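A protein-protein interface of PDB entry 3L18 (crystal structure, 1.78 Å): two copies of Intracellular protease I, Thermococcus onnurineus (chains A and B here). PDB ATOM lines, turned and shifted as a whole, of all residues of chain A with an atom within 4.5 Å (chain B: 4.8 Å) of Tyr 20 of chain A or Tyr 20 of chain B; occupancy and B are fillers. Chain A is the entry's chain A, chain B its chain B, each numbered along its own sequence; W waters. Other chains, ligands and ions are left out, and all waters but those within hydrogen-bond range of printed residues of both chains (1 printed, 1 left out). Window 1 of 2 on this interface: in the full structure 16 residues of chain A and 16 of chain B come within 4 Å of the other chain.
NE of Arg 24 of chain B lies within salt-bridge range of OE2 of Glu 27 of chain A.
The guanidinium group (NE) of Arg 24 of chain A sits close to the guanidinium group (NE) of Arg 24 of chain B (3.4 Å).
N of Arg 24 of chain B sits at hydrogen-bond distance from OH of Tyr 20 of chain A.
The side-chain hydroxyl (OH) of Tyr 20 of chain B sits at hydrogen-bond distance from the backbone NH (N) of Arg 24 of chain A (3.3 Å).
NE of Arg 24 of chain A lies within salt-bridge range of OE2 of Glu 27 of chain B (2.8 Å).
The backbone carbonyl oxygen of Ile 19 of chain A is in hydrogen-bond range of a ring nitrogen (ND1) of His 23 of chain A, at 3.4 Å.
NH1 of Arg 24 of chain B is in salt-bridge range of OE2 of Glu 27 of chain B, 3.6 Å away.
A ring nitrogen (ND1) of His 23 of chain B lies within hydrogen-bond range of the backbone carbonyl oxygen (O) of Ile 19 of chain B, at 3.3 Å.
OE2 of Glu 27 of chain A lies within salt-bridge range of NH1 of Arg 24 of chain A, 3.4 Å away.
CD2 of Leu 16 of chain B touches CD2 of Leu 16 of chain A (3.7 Å).
CG2 of Ile 19 of chain B touches CD2 of Leu 16 of chain A (3.7 Å).
Ile 19 of chain A touches Leu 16 of chain B (CG2 to CD1, 3.9 Å).
CD1 of Tyr 20 of chain A touches CD1 of Tyr 20 of chain B, 3.3 Å away.
C of His 23 of chain B touches OH of Tyr 20 of chain A, at 3.4 Å.
CB of Leu 156 of chain B touches CD2 of His 23 of chain A, at 3.6 Å.
Tyr 157 of chain B touches His 23 of chain A (N to CD2, 3.0 Å).
His 23 of chain B touches Leu 156 of chain A.
N of Tyr 157 of chain A touches CD2 of His 23 of chain B, at 3.1 Å.
CB of Glu 27 of chain B touches O of Tyr 157 of chain A (3.95 Å).
Tyr 20 of chain A touches just these residues of chain B: Tyr 20, His 23 and Arg 24.
Tyr 20 of chain B touches just these residues of chain A: Tyr 20 (3.3 Å), His 23 (3.5 Å) and Arg 24 (3.3 Å).
Of the printed residues of chain B, Leu 156 of chain A touches His 23.
Of the printed residues of chain B, Ile 19 of chain A touches Leu 16.
Printed residues of chain B within 4 Å of Tyr 157 of chain A: His 23 (3.1 Å) and Glu 27 (3.95 Å).
Met 160 of chain A touches none of the printed residues of chain B.
The nearest residue of chain B that does not touch Tyr 20 of chain A is Glu 27 of chain B (4.1 Å).
The nearest printed residue of chain B that does not touch Leu 16 of chain A is Asp 15 of chain B (5.1 Å).
Along chain B the printed residues that touch a printed residue of chain A span positions 16 to 157.
Hydrophobic or aromatic side chains of chain A that line the printed part of chain B: Leu 16, Ile 19, Tyr 20, His 23, Leu 156 and Tyr 157.
Leu 16 of chain B touches its own counterpart, Leu 16 of chain A.
Leu 16 of chain A touches Ile 19 of chain B, and with the chains exchanged Ile 19 of chain A touches Leu 16 of chain B.
Tyr 20 of chain A touches its own counterpart, Tyr 20 of chain B.
His 23 of chain A touches Leu 156 of chain B, and with the chains exchanged Leu 156 of chain A touches His 23 of chain B.
Of the 17 pairs that touch across the chains among the printed residues, 17 have their exchanged pair printed and touching as well.
Water W1 lies within hydrogen-bond range of the side-chain hydroxyl of Tyr 20 of chain B (2.5 Å), the side-chain carboxylate of Glu 27 of chain A (2.6 Å) and the backbone carbonyl oxygen of Tyr 157 of chain B (3.0 Å).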
ATOM      1  N   LEU A  16      10.855  33.176   3.043  1.00  0.00           N
ATOM      2  CA  LEU A  16      10.096  31.955   2.772  1.00  0.00           C
ATOM      3  C   LEU A  16       9.553  31.930   1.336  1.00  0.00           C
ATOM      4  O   LEU A  16       9.527  30.881   0.696  1.00  0.00           O
ATOM      5  CB  LEU A  16       8.935  31.801   3.773  1.00  0.00           C
ATOM      6  CG  LEU A  16       9.233  31.433   5.230  1.00  0.00           C
ATOM      7  CD1 LEU A  16       7.959  31.617   6.045  1.00  0.00           C
ATOM      8  CD2 LEU A  16       9.703  29.982   5.338  1.00  0.00           C
ATOM      9  N   LEU A  18      10.724  33.174  -1.448  1.00  0.00           N
ATOM     10  CA  LEU A  18      11.711  32.792  -2.460  1.00  0.00           C
ATOM     11  C   LEU A  18      12.226  31.376  -2.225  1.00  0.00           C
ATOM     12  O   LEU A  18      12.361  30.585  -3.159  1.00  0.00           O
ATOM     13  CB  LEU A  18      12.884  33.764  -2.472  1.00  0.00           C
ATOM     14  CG  LEU A  18      14.039  33.399  -3.437  1.00  0.00           C
ATOM     15  CD1 LEU A  18      13.568  33.234  -4.853  1.00  0.00           C
ATOM     16  CD2 LEU A  18      15.067  34.461  -3.407  1.00  0.00           C
ATOM     17  N   ILE A  19      12.547  31.064  -0.978  1.00  0.00           N
ATOM     18  CA  ILE A  19      13.248  29.822  -0.678  1.00  0.00           C
ATOM     19  C   ILE A  19      12.337  28.587  -0.769  1.00  0.00           C
ATOM     20  O   ILE A  19      12.770  27.536  -1.229  1.00  0.00           O
ATOM     21  CB  ILE A  19      13.991  29.922   0.667  1.00  0.00           C
ATOM     22  CG1 ILE A  19      15.076  31.026   0.592  1.00  0.00           C
ATOM     23  CG2 ILE A  19      14.597  28.547   1.064  1.00  0.00           C
ATOM     24  CD1 ILE A  19      15.695  31.425   1.971  1.00  0.00           C
ATOM     25  N   TYR A  20      11.083  28.704  -0.328  1.00  0.00           N
ATOM     26  CA  TYR A  20      10.128  27.599  -0.462  1.00  0.00           C
ATOM     27  C   TYR A  20       9.942  27.134  -1.932  1.00  0.00           C
ATOM     28  O   TYR A  20      10.188  25.968  -2.230  1.00  0.00           O
ATOM     29  CB  TYR A  20       8.780  27.942   0.223  1.00  0.00           C
ATOM     30  CG  TYR A  20       7.818  26.787   0.234  1.00  0.00           C
ATOM     31  CD1 TYR A  20       7.812  25.865   1.291  1.00  0.00           C
ATOM     32  CD2 TYR A  20       6.931  26.587  -0.826  1.00  0.00           C
ATOM     33  CE1 TYR A  20       6.964  24.783   1.288  1.00  0.00           C
ATOM     34  CE2 TYR A  20       6.058  25.493  -0.829  1.00  0.00           C
ATOM     35  CZ  TYR A  20       6.081  24.599   0.235  1.00  0.00           C
ATOM     36  OH  TYR A  20       5.215  23.517   0.244  1.00  0.00           O
ATOM     37  N   PRO A  21       9.545  28.042  -2.859  1.00  0.00           N
ATOM     38  CA  PRO A  21       9.399  27.574  -4.246  1.00  0.00           C
ATOM     39  C   PRO A  21      10.718  27.103  -4.896  1.00  0.00           C
ATOM     40  O   PRO A  21      10.691  26.187  -5.737  1.00  0.00           O
ATOM     41  CB  PRO A  21       8.802  28.779  -4.968  1.00  0.00           C
ATOM     42  CG  PRO A  21       9.270  29.966  -4.175  1.00  0.00           C
ATOM     43  CD  PRO A  21       9.198  29.465  -2.734  1.00  0.00           C
ATOM     44  N   LEU A  22      11.863  27.664  -4.497  1.00  0.00           N
ATOM     45  CA  LEU A  22      13.137  27.180  -5.057  1.00  0.00           C
ATOM     46  C   LEU A  22      13.290  25.688  -4.787  1.00  0.00           C
ATOM     47  O   LEU A  22      13.508  24.902  -5.707  1.00  0.00           O
ATOM     48  CB  LEU A  22      14.344  27.952  -4.498  1.00  0.00           C
ATOM     49  CG  LEU A  22      14.638  29.330  -5.116  1.00  0.00           C
ATOM     50  CD1 LEU A  22      15.629  30.078  -4.245  1.00  0.00           C
ATOM     51  CD2 LEU A  22      15.200  29.156  -6.520  1.00  0.00           C
ATOM     52  N   HIS A  23      13.164  25.297  -3.522  1.00  0.00           N
ATOM     53  CA  HIS A  23      13.294  23.900  -3.134  1.00  0.00           C
ATOM     54  C   HIS A  23      12.149  23.037  -3.636  1.00  0.00           C
ATOM     55  O   HIS A  23      12.372  21.924  -4.097  1.00  0.00           O
ATOM     56  CB  HIS A  23      13.434  23.764  -1.618  1.00  0.00           C
ATOM     57  CG  HIS A  23      14.826  24.007  -1.122  1.00  0.00           C
ATOM     58  ND1 HIS A  23      15.270  25.257  -0.737  1.00  0.00           N
ATOM     59  CD2 HIS A  23      15.871  23.167  -0.952  1.00  0.00           C
ATOM     60  CE1 HIS A  23      16.532  25.172  -0.348  1.00  0.00           C
ATOM     61  NE2 HIS A  23      16.922  23.917  -0.476  1.00  0.00           N
ATOM     62  N   ARG A  24      10.916  23.531  -3.538  1.00  0.00           N
ATOM     63  CA  ARG A  24       9.759  22.740  -3.977  1.00  0.00           C
ATOM     64  C   ARG A  24       9.835  22.393  -5.454  1.00  0.00           C
ATOM     65  O   ARG A  24       9.515  21.269  -5.866  1.00  0.00           O
ATOM     66  CB  ARG A  24       8.463  23.501  -3.710  1.00  0.00           C
ATOM     67  CG  ARG A  24       7.185  22.744  -4.131  1.00  0.00           C
ATOM     68  CD  ARG A  24       7.013  21.421  -3.354  1.00  0.00           C
ATOM     69  NE  ARG A  24       5.900  20.632  -3.905  1.00  0.00           N
ATOM     70  CZ  ARG A  24       6.016  19.712  -4.862  1.00  0.00           C
ATOM     71  NH1 ARG A  24       7.210  19.425  -5.379  1.00  0.00           N
ATOM     72  NH2 ARG A  24       4.935  19.051  -5.297  1.00  0.00           N
ATOM     73  N   GLU A  27      12.701  19.981  -6.211  1.00  0.00           N
ATOM     74  CA  GLU A  27      12.311  18.610  -5.837  1.00  0.00           C
ATOM     75  C   GLU A  27      11.817  17.835  -7.054  1.00  0.00           C
ATOM     76  O   GLU A  27      12.089  16.659  -7.203  1.00  0.00           O
ATOM     77  CB  GLU A  27      11.214  18.625  -4.763  1.00  0.00           C
ATOM     78  CG  GLU A  27      10.579  17.258  -4.536  1.00  0.00           C
ATOM     79  CD  GLU A  27       9.404  17.288  -3.593  1.00  0.00           C
ATOM     80  OE1 GLU A  27       8.669  16.280  -3.541  1.00  0.00           O
ATOM     81  OE2 GLU A  27       9.221  18.310  -2.914  1.00  0.00           O
ATOM     82  N   LEU A 156       1.709  29.178   1.353  1.00  0.00           N
ATOM     83  CA  LEU A 156       2.751  28.452   0.596  1.00  0.00           C
ATOM     84  C   LEU A 156       2.327  27.060   0.132  1.00  0.00           C
ATOM     85  O   LEU A 156       2.549  26.694  -1.013  1.00  0.00           O
ATOM     86  CB  LEU A 156       4.065  28.360   1.371  1.00  0.00           C
ATOM     87  CG  LEU A 156       4.823  29.679   1.594  1.00  0.00           C
ATOM     88  CD1 LEU A 156       5.923  29.485   2.691  1.00  0.00           C
ATOM     89  CD2 LEU A 156       5.400  30.324   0.295  1.00  0.00           C
ATOM     90  N   TYR A 157       1.716  26.280   1.020  1.00  0.00           N
ATOM     91  CA  TYR A 157       1.297  24.923   0.641  1.00  0.00           C
ATOM     92  C   TYR A 157       0.381  24.924  -0.594  1.00  0.00           C
ATOM     93  O   TYR A 157       0.648  24.216  -1.565  1.00  0.00           O
ATOM     94  CB  TYR A 157       0.622  24.212   1.810  1.00  0.00           C
ATOM     95  CG  TYR A 157      -0.794  24.659   2.101  1.00  0.00           C
ATOM     96  CD1 TYR A 157      -1.891  23.858   1.730  1.00  0.00           C
ATOM     97  CD2 TYR A 157      -1.041  25.859   2.768  1.00  0.00           C
ATOM     98  CE1 TYR A 157      -3.204  24.268   2.007  1.00  0.00           C
ATOM     99  CE2 TYR A 157      -2.351  26.284   3.031  1.00  0.00           C
ATOM    100  CZ  TYR A 157      -3.413  25.469   2.655  1.00  0.00           C
ATOM    101  OH  TYR A 157      -4.680  25.880   2.946  1.00  0.00           O
ATOM    102  N   MET A 160       2.225  26.479  -4.219  1.00  0.00           N
ATOM    103  CA  MET A 160       2.980  25.507  -5.009  1.00  0.00           C
ATOM    104  C   MET A 160       2.178  24.242  -5.335  1.00  0.00           C
ATOM    105  O   MET A 160       2.406  23.621  -6.375  1.00  0.00           O
ATOM    106  CB  MET A 160       4.315  25.170  -4.332  1.00  0.00           C
ATOM    107  CG  MET A 160       5.358  26.313  -4.466  1.00  0.00           C
ATOM    108  SD  MET A 160       5.798  26.721  -6.184  1.00  0.00           S
ATOM    109  CE  MET A 160       5.028  28.305  -6.400  1.00  0.00           C
ATOM    110  N   ASP B  15      14.009  28.376  11.222  1.00  0.00           N
ATOM    111  CA  ASP B  15      12.716  28.727  10.630  1.00  0.00           C
ATOM    112  C   ASP B  15      12.375  27.866   9.433  1.00  0.00           C
ATOM    113  O   ASP B  15      11.295  27.297   9.370  1.00  0.00           O
ATOM    114  CB  ASP B  15      12.679  30.219  10.258  1.00  0.00           C
ATOM    115  CG  ASP B  15      13.069  31.112  11.424  1.00  0.00           C
ATOM    116  OD1 ASP B  15      14.121  30.852  12.016  1.00  0.00           O
ATOM    117  OD2 ASP B  15      12.335  32.074  11.748  1.00  0.00           O
ATOM    118  N   LEU B  16      13.288  27.761   8.476  1.00  0.00           N
ATOM    119  CA  LEU B  16      12.956  27.010   7.260  1.00  0.00           C
ATOM    120  C   LEU B  16      12.752  25.536   7.552  1.00  0.00           C
ATOM    121  O   LEU B  16      11.963  24.881   6.893  1.00  0.00           O
ATOM    122  CB  LEU B  16      14.059  27.143   6.200  1.00  0.00           C
ATOM    123  CG  LEU B  16      14.351  28.533   5.642  1.00  0.00           C
ATOM    124  CD1 LEU B  16      15.663  28.486   4.852  1.00  0.00           C
ATOM    125  CD2 LEU B  16      13.205  29.006   4.787  1.00  0.00           C
ATOM    126  N   GLU B  17      13.486  24.996   8.515  1.00  0.00           N
ATOM    127  CA  GLU B  17      13.430  23.554   8.765  1.00  0.00           C
ATOM    128  C   GLU B  17      12.111  23.111   9.384  1.00  0.00           C
ATOM    129  O   GLU B  17      11.759  21.931   9.299  1.00  0.00           O
ATOM    130  CB  GLU B  17      14.595  23.131   9.655  1.00  0.00           C
ATOM    131  CG  GLU B  17      15.940  23.473   9.020  1.00  0.00           C
ATOM    132  CD  GLU B  17      17.111  23.104   9.906  1.00  0.00           C
ATOM    133  OE1 GLU B  17      16.876  22.649  11.049  1.00  0.00           O
ATOM    134  OE2 GLU B  17      18.266  23.303   9.457  1.00  0.00           O
ATOM    135  N   LEU B  18      11.395  24.035  10.022  1.00  0.00           N
ATOM    136  CA  LEU B  18      10.062  23.709  10.534  1.00  0.00           C
ATOM    137  C   LEU B  18       8.993  24.077   9.507  1.00  0.00           C
ATOM    138  O   LEU B  18       8.086  23.297   9.211  1.00  0.00           O
ATOM    139  CB  LEU B  18       9.771  24.430  11.863  1.00  0.00           C
ATOM    140  CG  LEU B  18       8.349  24.303  12.477  1.00  0.00           C
ATOM    141  CD1 LEU B  18       7.900  22.851  12.678  1.00  0.00           C
ATOM    142  CD2 LEU B  18       8.292  25.052  13.817  1.00  0.00           C
ATOM    143  N   ILE B  19       9.117  25.268   8.955  1.00  0.00           N
ATOM    144  CA  ILE B  19       8.062  25.817   8.100  1.00  0.00           C
ATOM    145  C   ILE B  19       8.021  25.159   6.711  1.00  0.00           C
ATOM    146  O   ILE B  19       6.941  24.929   6.171  1.00  0.00           O
ATOM    147  CB  ILE B  19       8.174  27.344   8.014  1.00  0.00           C
ATOM    148  CG1 ILE B  19       7.975  27.969   9.406  1.00  0.00           C
ATOM    149  CG2 ILE B  19       7.166  27.937   7.033  1.00  0.00           C
ATOM    150  CD1 ILE B  19       8.329  29.430   9.448  1.00  0.00           C
ATOM    151  N   TYR B  20       9.179  24.813   6.150  1.00  0.00           N
ATOM    152  CA  TYR B  20       9.191  24.127   4.856  1.00  0.00           C
ATOM    153  C   TYR B  20       8.401  22.788   4.875  1.00  0.00           C
ATOM    154  O   TYR B  20       7.494  22.593   4.050  1.00  0.00           O
ATOM    155  CB  TYR B  20      10.626  23.940   4.311  1.00  0.00           C
ATOM    156  CG  TYR B  20      10.640  23.312   2.929  1.00  0.00           C
ATOM    157  CD1 TYR B  20      10.530  24.099   1.785  1.00  0.00           C
ATOM    158  CD2 TYR B  20      10.724  21.921   2.769  1.00  0.00           C
ATOM    159  CE1 TYR B  20      10.514  23.521   0.518  1.00  0.00           C
ATOM    160  CE2 TYR B  20      10.701  21.336   1.500  1.00  0.00           C
ATOM    161  CZ  TYR B  20      10.618  22.146   0.384  1.00  0.00           C
ATOM    162  OH  TYR B  20      10.619  21.559  -0.872  1.00  0.00           O
ATOM    163  N   PRO B  21       8.732  21.864   5.805  1.00  0.00           N
ATOM    164  CA  PRO B  21       7.993  20.599   5.857  1.00  0.00           C
ATOM    165  C   PRO B  21       6.533  20.743   6.275  1.00  0.00           C
ATOM    166  O   PRO B  21       5.714  19.956   5.843  1.00  0.00           O
ATOM    167  CB  PRO B  21       8.786  19.761   6.884  1.00  0.00           C
ATOM    168  CG  PRO B  21       9.506  20.766   7.730  1.00  0.00           C
ATOM    169  CD  PRO B  21       9.858  21.875   6.759  1.00  0.00           C
ATOM    170  N   LEU B  22       6.190  21.748   7.084  1.00  0.00           N
ATOM    171  CA  LEU B  22       4.773  21.948   7.433  1.00  0.00           C
ATOM    172  C   LEU B  22       3.934  22.136   6.175  1.00  0.00           C
ATOM    173  O   LEU B  22       2.903  21.473   5.979  1.00  0.00           O
ATOM    174  CB  LEU B  22       4.586  23.155   8.374  1.00  0.00           C
ATOM    175  CG  LEU B  22       4.874  22.944   9.871  1.00  0.00           C
ATOM    176  CD1 LEU B  22       4.962  24.290  10.618  1.00  0.00           C
ATOM    177  CD2 LEU B  22       3.818  22.097  10.502  1.00  0.00           C
ATOM    178  N   HIS B  23       4.384  23.038   5.311  1.00  0.00           N
ATOM    179  CA  HIS B  23       3.647  23.335   4.092  1.00  0.00           C
ATOM    180  C   HIS B  23       3.780  22.226   3.069  1.00  0.00           C
ATOM    181  O   HIS B  23       2.810  21.887   2.391  1.00  0.00           O
ATOM    182  CB  HIS B  23       4.148  24.652   3.498  1.00  0.00           C
ATOM    183  CG  HIS B  23       3.563  25.854   4.169  1.00  0.00           C
ATOM    184  ND1 HIS B  23       4.207  26.538   5.178  1.00  0.00           N
ATOM    185  CD2 HIS B  23       2.372  26.474   3.994  1.00  0.00           C
ATOM    186  CE1 HIS B  23       3.442  27.539   5.588  1.00  0.00           C
ATOM    187  NE2 HIS B  23       2.329  27.529   4.875  1.00  0.00           N
ATOM    188  N   ARG B  24       4.983  21.675   2.943  1.00  0.00           N
ATOM    189  CA  ARG B  24       5.213  20.629   1.957  1.00  0.00           C
ATOM    190  C   ARG B  24       4.332  19.415   2.230  1.00  0.00           C
ATOM    191  O   ARG B  24       3.730  18.846   1.314  1.00  0.00           O
ATOM    192  CB  ARG B  24       6.696  20.235   1.879  1.00  0.00           C
ATOM    193  CG  ARG B  24       6.937  19.070   0.919  1.00  0.00           C
ATOM    194  CD  ARG B  24       6.723  19.544  -0.514  1.00  0.00           C
ATOM    195  NE  ARG B  24       6.811  18.459  -1.504  1.00  0.00           N
ATOM    196  CZ  ARG B  24       5.800  17.670  -1.868  1.00  0.00           C
ATOM    197  NH1 ARG B  24       4.590  17.813  -1.334  1.00  0.00           N
ATOM    198  NH2 ARG B  24       6.006  16.726  -2.786  1.00  0.00           N
ATOM    199  N   GLU B  27       0.576  20.211   1.664  1.00  0.00           N
ATOM    200  CA  GLU B  27       0.305  20.182   0.218  1.00  0.00           C
ATOM    201  C   GLU B  27      -0.256  18.827  -0.207  1.00  0.00           C
ATOM    202  O   GLU B  27      -1.196  18.761  -1.002  1.00  0.00           O
ATOM    203  CB  GLU B  27       1.563  20.488  -0.616  1.00  0.00           C
ATOM    204  CG  GLU B  27       1.371  20.026  -2.044  1.00  0.00           C
ATOM    205  CD  GLU B  27       2.531  20.294  -2.955  1.00  0.00           C
ATOM    206  OE1 GLU B  27       2.479  19.768  -4.096  1.00  0.00           O
ATOM    207  OE2 GLU B  27       3.471  21.014  -2.547  1.00  0.00           O
ATOM    208  N   LEU B 156      16.761  20.819   1.961  1.00  0.00           N
ATOM    209  CA  LEU B 156      15.293  20.732   2.063  1.00  0.00           C
ATOM    210  C   LEU B 156      14.595  20.035   0.899  1.00  0.00           C
ATOM    211  O   LEU B 156      13.799  19.132   1.134  1.00  0.00           O
ATOM    212  CB  LEU B 156      14.668  22.103   2.280  1.00  0.00           C
ATOM    213  CG  LEU B 156      14.945  22.812   3.605  1.00  0.00           C
ATOM    214  CD1 LEU B 156      14.480  24.240   3.443  1.00  0.00           C
ATOM    215  CD2 LEU B 156      14.264  22.108   4.792  1.00  0.00           C
ATOM    216  N   TYR B 157      14.909  20.422  -0.344  1.00  0.00           N
ATOM    217  CA  TYR B 157      14.286  19.785  -1.510  1.00  0.00           C
ATOM    218  C   TYR B 157      14.427  18.258  -1.467  1.00  0.00           C
ATOM    219  O   TYR B 157      13.453  17.540  -1.669  1.00  0.00           O
ATOM    220  CB  TYR B 157      14.870  20.336  -2.821  1.00  0.00           C
ATOM    221  CG  TYR B 157      16.241  19.818  -3.204  1.00  0.00           C
ATOM    222  CD1 TYR B 157      16.386  18.842  -4.213  1.00  0.00           C
ATOM    223  CD2 TYR B 157      17.397  20.307  -2.587  1.00  0.00           C
ATOM    224  CE1 TYR B 157      17.639  18.348  -4.573  1.00  0.00           C
ATOM    225  CE2 TYR B 157      18.668  19.814  -2.948  1.00  0.00           C
ATOM    226  CZ  TYR B 157      18.773  18.843  -3.942  1.00  0.00           C
ATOM    227  OH  TYR B 157      20.012  18.360  -4.322  1.00  0.00           O
ATOM    228  N   MET B 160      12.518  16.460   1.911  1.00  0.00           N
ATOM    229  CA  MET B 160      11.096  16.178   1.773  1.00  0.00           C
ATOM    230  C   MET B 160      10.756  15.339   0.541  1.00  0.00           C
ATOM    231  O   MET B 160       9.757  14.609   0.550  1.00  0.00           O
ATOM    232  CB  MET B 160      10.273  17.480   1.824  1.00  0.00           C
ATOM    233  CG  MET B 160      10.161  18.071   3.238  1.00  0.00           C
ATOM    234  SD  MET B 160       9.273  16.926   4.330  1.00  0.00           S
ATOM    235  CE  MET B 160      10.540  16.389   5.473  1.00  0.00           C
HETATM  236  O   HOH W   1      10.925  19.047  -1.046  1.00  0.00           O
